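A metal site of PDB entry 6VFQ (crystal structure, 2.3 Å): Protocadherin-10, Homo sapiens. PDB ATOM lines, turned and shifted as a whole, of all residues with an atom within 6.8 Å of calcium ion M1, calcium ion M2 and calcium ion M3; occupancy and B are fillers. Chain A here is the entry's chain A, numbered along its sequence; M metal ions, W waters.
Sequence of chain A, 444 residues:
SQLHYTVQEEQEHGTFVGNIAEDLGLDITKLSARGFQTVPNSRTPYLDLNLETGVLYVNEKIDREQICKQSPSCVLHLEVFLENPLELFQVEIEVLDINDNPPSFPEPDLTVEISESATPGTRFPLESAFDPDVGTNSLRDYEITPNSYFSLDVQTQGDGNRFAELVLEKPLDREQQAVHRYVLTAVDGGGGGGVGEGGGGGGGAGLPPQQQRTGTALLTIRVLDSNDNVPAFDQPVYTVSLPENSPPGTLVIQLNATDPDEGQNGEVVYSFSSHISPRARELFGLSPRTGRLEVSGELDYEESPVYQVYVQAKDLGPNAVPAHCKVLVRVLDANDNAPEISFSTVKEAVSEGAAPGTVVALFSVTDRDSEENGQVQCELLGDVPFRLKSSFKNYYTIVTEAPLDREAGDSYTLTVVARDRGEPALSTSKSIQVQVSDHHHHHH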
ATOM      1  N   GLU A 116      -9.367  31.077  13.870  1.00  0.00           N
ATOM      2  CA  GLU A 116      -9.959  29.773  14.114  1.00  0.00           C
ATOM      3  C   GLU A 116      -9.245  29.001  15.206  1.00  0.00           C
ATOM      4  O   GLU A 116      -9.774  28.010  15.708  1.00  0.00           O
ATOM      5  CB  GLU A 116     -10.001  28.947  12.825  1.00  0.00           C
ATOM      6  CG  GLU A 116      -8.674  28.350  12.399  1.00  0.00           C
ATOM      7  CD  GLU A 116      -8.766  27.512  11.116  1.00  0.00           C
ATOM      8  OE1 GLU A 116      -9.704  26.703  10.973  1.00  0.00           O
ATOM      9  OE2 GLU A 116      -7.877  27.677  10.265  1.00  0.00           O
ATOM     10  N   LEU A 172     -13.962  27.370  16.509  1.00  0.00           N
ATOM     11  CA  LEU A 172     -14.332  27.636  15.131  1.00  0.00           C
ATOM     12  C   LEU A 172     -13.426  26.834  14.194  1.00  0.00           C
ATOM     13  O   LEU A 172     -12.319  26.429  14.546  1.00  0.00           O
ATOM     14  CB  LEU A 172     -14.225  29.125  14.820  1.00  0.00           C
ATOM     15  CG  LEU A 172     -14.916  30.131  15.721  1.00  0.00           C
ATOM     16  CD1 LEU A 172     -14.151  31.402  15.671  1.00  0.00           C
ATOM     17  CD2 LEU A 172     -16.328  30.351  15.244  1.00  0.00           C
ATOM     18  N   ASP A 173     -13.894  26.646  12.959  1.00  0.00           N
ATOM     19  CA  ASP A 173     -13.155  25.905  11.939  1.00  0.00           C
ATOM     20  C   ASP A 173     -13.379  26.613  10.622  1.00  0.00           C
ATOM     21  O   ASP A 173     -14.445  26.453   9.999  1.00  0.00           O
ATOM     22  CB  ASP A 173     -13.609  24.452  11.866  1.00  0.00           C
ATOM     23  CG  ASP A 173     -12.835  23.611  10.827  1.00  0.00           C
ATOM     24  OD1 ASP A 173     -11.740  24.022  10.348  1.00  0.00           O
ATOM     25  OD2 ASP A 173     -13.343  22.510  10.496  1.00  0.00           O
ATOM     26  N   ARG A 174     -12.383  27.381  10.176  1.00  0.00           N
ATOM     27  CA  ARG A 174     -12.557  28.154   8.945  1.00  0.00           C
ATOM     28  C   ARG A 174     -12.842  27.240   7.768  1.00  0.00           C
ATOM     29  O   ARG A 174     -13.599  27.605   6.858  1.00  0.00           O
ATOM     30  CB  ARG A 174     -11.313  28.971   8.658  1.00  0.00           C
ATOM     31  CG  ARG A 174     -11.456  29.887   7.482  1.00  0.00           C
ATOM     32  CD  ARG A 174     -10.091  30.303   6.955  1.00  0.00           C
ATOM     33  NE  ARG A 174      -9.482  29.148   6.284  1.00  0.00           N
ATOM     34  CZ  ARG A 174      -9.838  28.734   5.075  1.00  0.00           C
ATOM     35  NH1 ARG A 174     -10.765  29.390   4.385  1.00  0.00           N
ATOM     36  NH2 ARG A 174      -9.275  27.659   4.542  1.00  0.00           N
ATOM     37  N   GLU A 175     -12.197  26.065   7.761  1.00  0.00           N
ATOM     38  CA  GLU A 175     -12.357  25.118   6.674  1.00  0.00           C
ATOM     39  C   GLU A 175     -13.768  24.554   6.610  1.00  0.00           C
ATOM     40  O   GLU A 175     -14.153  23.974   5.594  1.00  0.00           O
ATOM     41  CB  GLU A 175     -11.333  23.972   6.842  1.00  0.00           C
ATOM     42  CG  GLU A 175      -9.896  24.319   6.408  1.00  0.00           C
ATOM     43  CD  GLU A 175      -9.109  25.230   7.351  1.00  0.00           C
ATOM     44  OE1 GLU A 175      -8.622  26.275   6.875  1.00  0.00           O
ATOM     45  OE2 GLU A 175      -8.922  24.897   8.542  1.00  0.00           O
ATOM     46  N   GLN A 176     -14.542  24.718   7.689  1.00  0.00           N
ATOM     47  CA  GLN A 176     -15.940  24.296   7.727  1.00  0.00           C
ATOM     48  C   GLN A 176     -16.906  25.436   7.470  1.00  0.00           C
ATOM     49  O   GLN A 176     -17.936  25.243   6.823  1.00  0.00           O
ATOM     50  CB  GLN A 176     -16.269  23.678   9.075  1.00  0.00           C
ATOM     51  CG  GLN A 176     -17.695  23.182   9.186  1.00  0.00           C
ATOM     52  CD  GLN A 176     -17.832  22.056  10.197  1.00  0.00           C
ATOM     53  OE1 GLN A 176     -16.831  21.567  10.740  1.00  0.00           O
ATOM     54  NE2 GLN A 176     -19.064  21.628  10.423  1.00  0.00           N
ATOM     55  N   LEU A 224     -10.482  33.730  10.678  1.00  0.00           N
ATOM     56  CA  LEU A 224      -9.165  33.841  10.064  1.00  0.00           C
ATOM     57  C   LEU A 224      -8.449  32.497  10.086  1.00  0.00           C
ATOM     58  O   LEU A 224      -8.503  31.751  11.074  1.00  0.00           O
ATOM     59  CB  LEU A 224      -8.327  34.885  10.803  1.00  0.00           C
ATOM     60  CG  LEU A 224      -8.526  36.314  10.329  1.00  0.00           C
ATOM     61  CD1 LEU A 224      -9.974  36.701  10.306  1.00  0.00           C
ATOM     62  CD2 LEU A 224      -7.731  37.245  11.249  1.00  0.00           C
ATOM     63  N   ASP A 225      -7.745  32.196   8.995  1.00  0.00           N
ATOM     64  CA  ASP A 225      -7.097  30.913   8.846  1.00  0.00           C
ATOM     65  C   ASP A 225      -5.897  30.747   9.775  1.00  0.00           C
ATOM     66  O   ASP A 225      -5.113  31.672   9.990  1.00  0.00           O
ATOM     67  CB  ASP A 225      -6.625  30.734   7.406  1.00  0.00           C
ATOM     68  CG  ASP A 225      -6.119  29.325   7.126  1.00  0.00           C
ATOM     69  OD1 ASP A 225      -6.819  28.345   7.467  1.00  0.00           O
ATOM     70  OD2 ASP A 225      -5.006  29.213   6.584  1.00  0.00           O
ATOM     71  N   SER A 226      -5.808  29.571  10.371  1.00  0.00           N
ATOM     72  CA  SER A 226      -4.571  29.060  10.945  1.00  0.00           C
ATOM     73  C   SER A 226      -4.089  27.871  10.129  1.00  0.00           C
ATOM     74  O   SER A 226      -4.857  27.228   9.405  1.00  0.00           O
ATOM     75  CB  SER A 226      -4.765  28.634  12.397  1.00  0.00           C
ATOM     76  OG  SER A 226      -5.393  27.365  12.452  1.00  0.00           O
ATOM     77  N   ASN A 227      -2.781  27.574  10.254  1.00  0.00           N
ATOM     78  CA  ASN A 227      -2.185  26.459   9.514  1.00  0.00           C
ATOM     79  C   ASN A 227      -2.347  25.178  10.320  1.00  0.00           C
ATOM     80  O   ASN A 227      -1.417  24.651  10.914  1.00  0.00           O
ATOM     81  CB  ASN A 227      -0.712  26.739   9.202  1.00  0.00           C
ATOM     82  CG  ASN A 227      -0.150  25.783   8.127  1.00  0.00           C
ATOM     83  OD1 ASN A 227      -0.895  25.133   7.409  1.00  0.00           O
ATOM     84  ND2 ASN A 227       1.164  25.705   8.022  1.00  0.00           N
ATOM     85  N   ASP A 228      -3.594  24.690  10.342  1.00  0.00           N
ATOM     86  CA  ASP A 228      -3.977  23.555  11.171  1.00  0.00           C
ATOM     87  C   ASP A 228      -4.279  22.295  10.368  1.00  0.00           C
ATOM     88  O   ASP A 228      -4.698  21.287  10.947  1.00  0.00           O
ATOM     89  CB  ASP A 228      -5.169  23.947  12.065  1.00  0.00           C
ATOM     90  CG  ASP A 228      -6.401  24.410  11.281  1.00  0.00           C
ATOM     91  OD1 ASP A 228      -6.308  24.827  10.103  1.00  0.00           O
ATOM     92  OD2 ASP A 228      -7.510  24.386  11.878  1.00  0.00           O
ATOM     93  N   ASN A 229      -4.068  22.311   9.045  1.00  0.00           N
ATOM     94  CA  ASN A 229      -4.177  21.112   8.234  1.00  0.00           C
ATOM     95  C   ASN A 229      -2.827  20.794   7.616  1.00  0.00           C
ATOM     96  O   ASN A 229      -2.152  21.681   7.075  1.00  0.00           O
ATOM     97  CB  ASN A 229      -5.196  21.263   7.118  1.00  0.00           C
ATOM     98  CG  ASN A 229      -6.599  21.232   7.634  1.00  0.00           C
ATOM     99  OD1 ASN A 229      -7.170  20.165   7.862  1.00  0.00           O
ATOM    100  ND2 ASN A 229      -7.178  22.433   7.856  1.00  0.00           N
ATOM    101  N   VAL A 230      -2.466  19.510   7.687  1.00  0.00           N
ATOM    102  CA  VAL A 230      -1.219  18.984   7.144  1.00  0.00           C
ATOM    103  C   VAL A 230      -1.523  18.458   5.754  1.00  0.00           C
ATOM    104  O   VAL A 230      -2.569  17.841   5.562  1.00  0.00           O
ATOM    105  CB  VAL A 230      -0.654  17.873   8.039  1.00  0.00           C
ATOM    106  CG1 VAL A 230       0.579  17.210   7.386  1.00  0.00           C
ATOM    107  CG2 VAL A 230      -0.358  18.457   9.432  1.00  0.00           C
ATOM    108  N   PRO A 231      -0.650  18.669   4.766  1.00  0.00           N
ATOM    109  CA  PRO A 231      -0.880  18.077   3.448  1.00  0.00           C
ATOM    110  C   PRO A 231      -1.056  16.566   3.559  1.00  0.00           C
ATOM    111  O   PRO A 231      -0.469  15.903   4.407  1.00  0.00           O
ATOM    112  CB  PRO A 231       0.381  18.441   2.667  1.00  0.00           C
ATOM    113  CG  PRO A 231       0.866  19.696   3.325  1.00  0.00           C
ATOM    114  CD  PRO A 231       0.558  19.525   4.780  1.00  0.00           C
ATOM    115  N   ASP A 259      -4.323  20.136   0.786  1.00  0.00           N
ATOM    116  CA  ASP A 259      -4.195  20.972   1.981  1.00  0.00           C
ATOM    117  C   ASP A 259      -5.288  22.028   1.903  1.00  0.00           C
ATOM    118  O   ASP A 259      -5.194  22.958   1.103  1.00  0.00           O
ATOM    119  CB  ASP A 259      -2.806  21.604   2.043  1.00  0.00           C
ATOM    120  CG  ASP A 259      -2.497  22.223   3.410  1.00  0.00           C
ATOM    121  OD1 ASP A 259      -3.358  22.901   4.027  1.00  0.00           O
ATOM    122  OD2 ASP A 259      -1.344  22.054   3.875  1.00  0.00           O
ATOM    123  N   PRO A 260      -6.346  21.916   2.703  1.00  0.00           N
ATOM    124  CA  PRO A 260      -7.464  22.867   2.595  1.00  0.00           C
ATOM    125  C   PRO A 260      -7.226  24.247   3.217  1.00  0.00           C
ATOM    126  O   PRO A 260      -8.121  25.092   3.122  1.00  0.00           O
ATOM    127  CB  PRO A 260      -8.593  22.151   3.320  1.00  0.00           C
ATOM    128  CG  PRO A 260      -7.884  21.272   4.320  1.00  0.00           C
ATOM    129  CD  PRO A 260      -6.619  20.838   3.669  1.00  0.00           C
ATOM    130  N   ASP A 261      -6.071  24.528   3.829  1.00  0.00           N
ATOM    131  CA  ASP A 261      -5.859  25.835   4.429  1.00  0.00           C
ATOM    132  C   ASP A 261      -5.859  26.916   3.362  1.00  0.00           C
ATOM    133  O   ASP A 261      -5.976  26.642   2.170  1.00  0.00           O
ATOM    134  CB  ASP A 261      -4.563  25.855   5.234  1.00  0.00           C
ATOM    135  CG  ASP A 261      -4.645  25.013   6.483  1.00  0.00           C
ATOM    136  OD1 ASP A 261      -5.713  25.008   7.114  1.00  0.00           O
ATOM    137  OD2 ASP A 261      -3.647  24.330   6.818  1.00  0.00           O
ATOM    138  N   GLU A 262      -5.697  28.160   3.794  1.00  0.00           N
ATOM    139  CA  GLU A 262      -5.780  29.335   2.936  1.00  0.00           C
ATOM    140  C   GLU A 262      -4.389  29.951   2.737  1.00  0.00           C
ATOM    141  O   GLU A 262      -3.519  29.823   3.591  1.00  0.00           O
ATOM    142  CB  GLU A 262      -6.733  30.354   3.575  1.00  0.00           C
ATOM    143  CG  GLU A 262      -6.840  31.687   2.903  1.00  0.00           C
ATOM    144  CD  GLU A 262      -7.792  32.614   3.661  1.00  0.00           C
ATOM    145  OE1 GLU A 262      -8.996  32.609   3.349  1.00  0.00           O
ATOM    146  OE2 GLU A 262      -7.330  33.323   4.589  1.00  0.00           O
ATOM    147  N   GLN A 264      -0.586  30.847   1.826  1.00  0.00           N
ATOM    148  CA  GLN A 264       0.628  30.049   1.955  1.00  0.00           C
ATOM    149  C   GLN A 264       0.390  28.813   2.818  1.00  0.00           C
ATOM    150  O   GLN A 264       0.962  27.752   2.554  1.00  0.00           O
ATOM    151  CB  GLN A 264       1.747  30.918   2.542  1.00  0.00           C
ATOM    152  CG  GLN A 264       2.138  32.117   1.659  1.00  0.00           C
ATOM    153  CD  GLN A 264       2.425  31.725   0.212  1.00  0.00           C
ATOM    154  OE1 GLN A 264       3.516  31.226  -0.126  1.00  0.00           O
ATOM    155  NE2 GLN A 264       1.423  31.904  -0.649  1.00  0.00           N
ATOM    156  N   ASN A 265      -0.476  28.923   3.844  1.00  0.00           N
ATOM    157  CA  ASN A 265      -0.811  27.771   4.671  1.00  0.00           C
ATOM    158  C   ASN A 265      -1.299  26.609   3.835  1.00  0.00           C
ATOM    159  O   ASN A 265      -1.179  25.452   4.251  1.00  0.00           O
ATOM    160  CB  ASN A 265      -1.892  28.122   5.698  1.00  0.00           C
ATOM    161  CG  ASN A 265      -1.453  29.191   6.644  1.00  0.00           C
ATOM    162  OD1 ASN A 265      -0.264  29.391   6.845  1.00  0.00           O
ATOM    163  ND2 ASN A 265      -2.415  29.899   7.228  1.00  0.00           N
ATOM    164  N   GLY A 266      -1.882  26.905   2.679  1.00  0.00           N
ATOM    165  CA  GLY A 266      -2.479  25.869   1.871  1.00  0.00           C
ATOM    166  C   GLY A 266      -1.734  25.563   0.583  1.00  0.00           C
ATOM    167  O   GLY A 266      -2.172  24.704  -0.181  1.00  0.00           O
ATOM    168  N   GLU A 267      -0.631  26.272   0.331  1.00  0.00           N
ATOM    169  CA  GLU A 267       0.194  26.031  -0.849  1.00  0.00           C
ATOM    170  C   GLU A 267       1.250  24.982  -0.538  1.00  0.00           C
ATOM    171  O   GLU A 267       2.006  25.122   0.435  1.00  0.00           O
ATOM    172  CB  GLU A 267       0.874  27.329  -1.317  1.00  0.00           C
ATOM    173  CG  GLU A 267      -0.020  28.300  -2.056  1.00  0.00           C
ATOM    174  CD  GLU A 267      -0.567  27.733  -3.364  1.00  0.00           C
ATOM    175  OE1 GLU A 267       0.186  27.054  -4.106  1.00  0.00           O
ATOM    176  OE2 GLU A 267      -1.766  27.957  -3.637  1.00  0.00           O
ATOM    177  N   VAL A 268       1.308  23.931  -1.371  1.00  0.00           N
ATOM    178  CA  VAL A 268       2.127  22.756  -1.115  1.00  0.00           C
ATOM    179  C   VAL A 268       3.280  22.702  -2.122  1.00  0.00           C
ATOM    180  O   VAL A 268       3.083  22.878  -3.331  1.00  0.00           O
ATOM    181  CB  VAL A 268       1.282  21.471  -1.212  1.00  0.00           C
ATOM    182  CG1 VAL A 268       2.143  20.262  -0.957  1.00  0.00           C
ATOM    183  CG2 VAL A 268       0.166  21.526  -0.242  1.00  0.00           C
ATOM    184  N   ASP A 315       3.514  22.353   3.303  1.00  0.00           N
ATOM    185  CA  ASP A 315       2.939  23.615   2.863  1.00  0.00           C
ATOM    186  C   ASP A 315       3.933  24.740   3.158  1.00  0.00           C
ATOM    187  O   ASP A 315       4.988  24.521   3.751  1.00  0.00           O
ATOM    188  CB  ASP A 315       1.557  23.839   3.469  1.00  0.00           C
ATOM    189  CG  ASP A 315       1.557  24.030   4.996  1.00  0.00           C
ATOM    190  OD1 ASP A 315       2.323  24.866   5.523  1.00  0.00           O
ATOM    191  OD2 ASP A 315       0.758  23.335   5.668  1.00  0.00           O
ATOM    192  N   LEU A 316       3.607  25.938   2.685  1.00  0.00           N
ATOM    193  CA  LEU A 316       4.483  27.084   2.798  1.00  0.00           C
ATOM    194  C   LEU A 316       4.151  27.998   3.987  1.00  0.00           C
ATOM    195  O   LEU A 316       4.656  29.127   4.064  1.00  0.00           O
ATOM    196  CB  LEU A 316       4.443  27.871   1.497  1.00  0.00           C
ATOM    197  CG  LEU A 316       5.046  27.185   0.271  1.00  0.00           C
ATOM    198  CD1 LEU A 316       4.733  27.948  -0.994  1.00  0.00           C
ATOM    199  CD2 LEU A 316       6.525  27.056   0.386  1.00  0.00           C
ATOM    200  N   GLY A 317       3.330  27.543   4.934  1.00  0.00           N
ATOM    201  CA  GLY A 317       2.958  28.372   6.071  1.00  0.00           C
ATOM    202  C   GLY A 317       3.907  28.211   7.256  1.00  0.00           C
ATOM    203  O   GLY A 317       4.814  27.375   7.248  1.00  0.00           O
ATOM    204  N   ALA A 320       4.785  24.622   9.504  1.00  0.00           N
ATOM    205  CA  ALA A 320       4.348  23.558   8.609  1.00  0.00           C
ATOM    206  C   ALA A 320       4.873  22.211   9.069  1.00  0.00           C
ATOM    207  O   ALA A 320       5.981  22.088   9.591  1.00  0.00           O
ATOM    208  CB  ALA A 320       4.814  23.850   7.186  1.00  0.00           C
HETATM  209 CA    CA M   1      -9.522  24.368  10.808  1.00  0.00          CA
HETATM  210 CA    CA M   2      -6.933  26.396   8.542  1.00  0.00          CA
HETATM  211 CA    CA M   3      -1.617  23.582   5.765  1.00  0.00          CA
HETATM  212  O   HOH W   1     -10.698  23.718  12.721  1.00  0.00           O
HETATM  213  O   HOH W   2      -8.887  22.148  10.202  1.00  0.00           O
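OD2 of Asp 225 is in hydrogen-bond range of ND2 of Asn 265, at 2.8 Å. The side-chain carboxylate (OD1) of Asp 225 sits close to the guanidinium group (NE) of Arg 174, 3.0 Å away. N of Glu 262 lies within hydrogen-bond range of OD2 of Asp 225 (3.1 Å). OD1 of Asp 228 sits close to ND2 of Asn 229. The side-chain carboxylate of Glu 116 sits close to the backbone NH of Arg 174. N of Glu 116 is in hydrogen-bond range of O of Leu 224 (3.0 Å). ND2 of Asn 229 lies close to OE2 of Glu 175, 3.1 Å away. The side-chain carboxylate of Glu 175 lies close to the guanidinium group of Arg 174, 2.8 Å away.
The nearest printed residue that does not touch calcium ion M1 is Arg 174 (4.2 Å).
Within 4 Å of calcium ion M2: Glu 116, Glu 175, Asp 225, Ser 226, Asp 228 and Asp 261. The nearest printed residue that does not touch calcium ion M2 is Asn 229 (4.03 Å).
Six residues have an atom within 4 Å of calcium ion M3: Asn 227, Asn 229, Asp 259, Asp 261, Asn 265 and Asp 315.
Calcium ion M1 is bound by OD2 of Asp 228, 2.3 Å away. OD1 of Asp 173 is bound to calcium ion M1 (2.3 Å). Water W1 is bound to calcium ion M1, 2.3 Å away. Calcium ion M1 is bound by OE1 of Glu 116 (2.3 Å). Water W2 is bound to calcium ion M1 (2.4 Å). Calcium ion M1 is bound by OE2 of Glu 175 (2.4 Å). Calcium ion M1 has six donor atoms within binding distance.
The side-chain carboxylate (OD1) of Asp 225 binds calcium ion M2, at 2.2 Å. OD1 of Asp 228 binds calcium ion M2 (2.3 Å). Calcium ion M2 is bound by OD1 of Asp 261, at 2.3 Å. Calcium ion M2 is bound by OE2 of Glu 116, at 2.3 Å. Calcium ion M2 is bound by the side-chain carboxylate (OE1) of Glu 175 (2.4 Å). Calcium ion M2 is bound by O of Ser 226 (2.4 Å). OE2 of Glu 175 binds calcium ion M2.
O of Asn 229 binds calcium ion M3. OD1 of Asn 227 is bound to calcium ion M3, at 2.4 Å. Calcium ion M3 is bound by the side-chain carboxylate (OD2) of Asp 315 (2.4 Å). The side-chain carboxylate (OD2) of Asp 261 is bound to calcium ion M3 (2.4 Å). O of Asn 265 binds calcium ion M3, 2.4 Å away. The side-chain carboxylate (OD2) of Asp 259 is bound to calcium ion M3. OD1 of Asp 259 binds calcium ion M3 (2.6 Å). Calcium ion M3 has seven donor atoms within binding distance.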
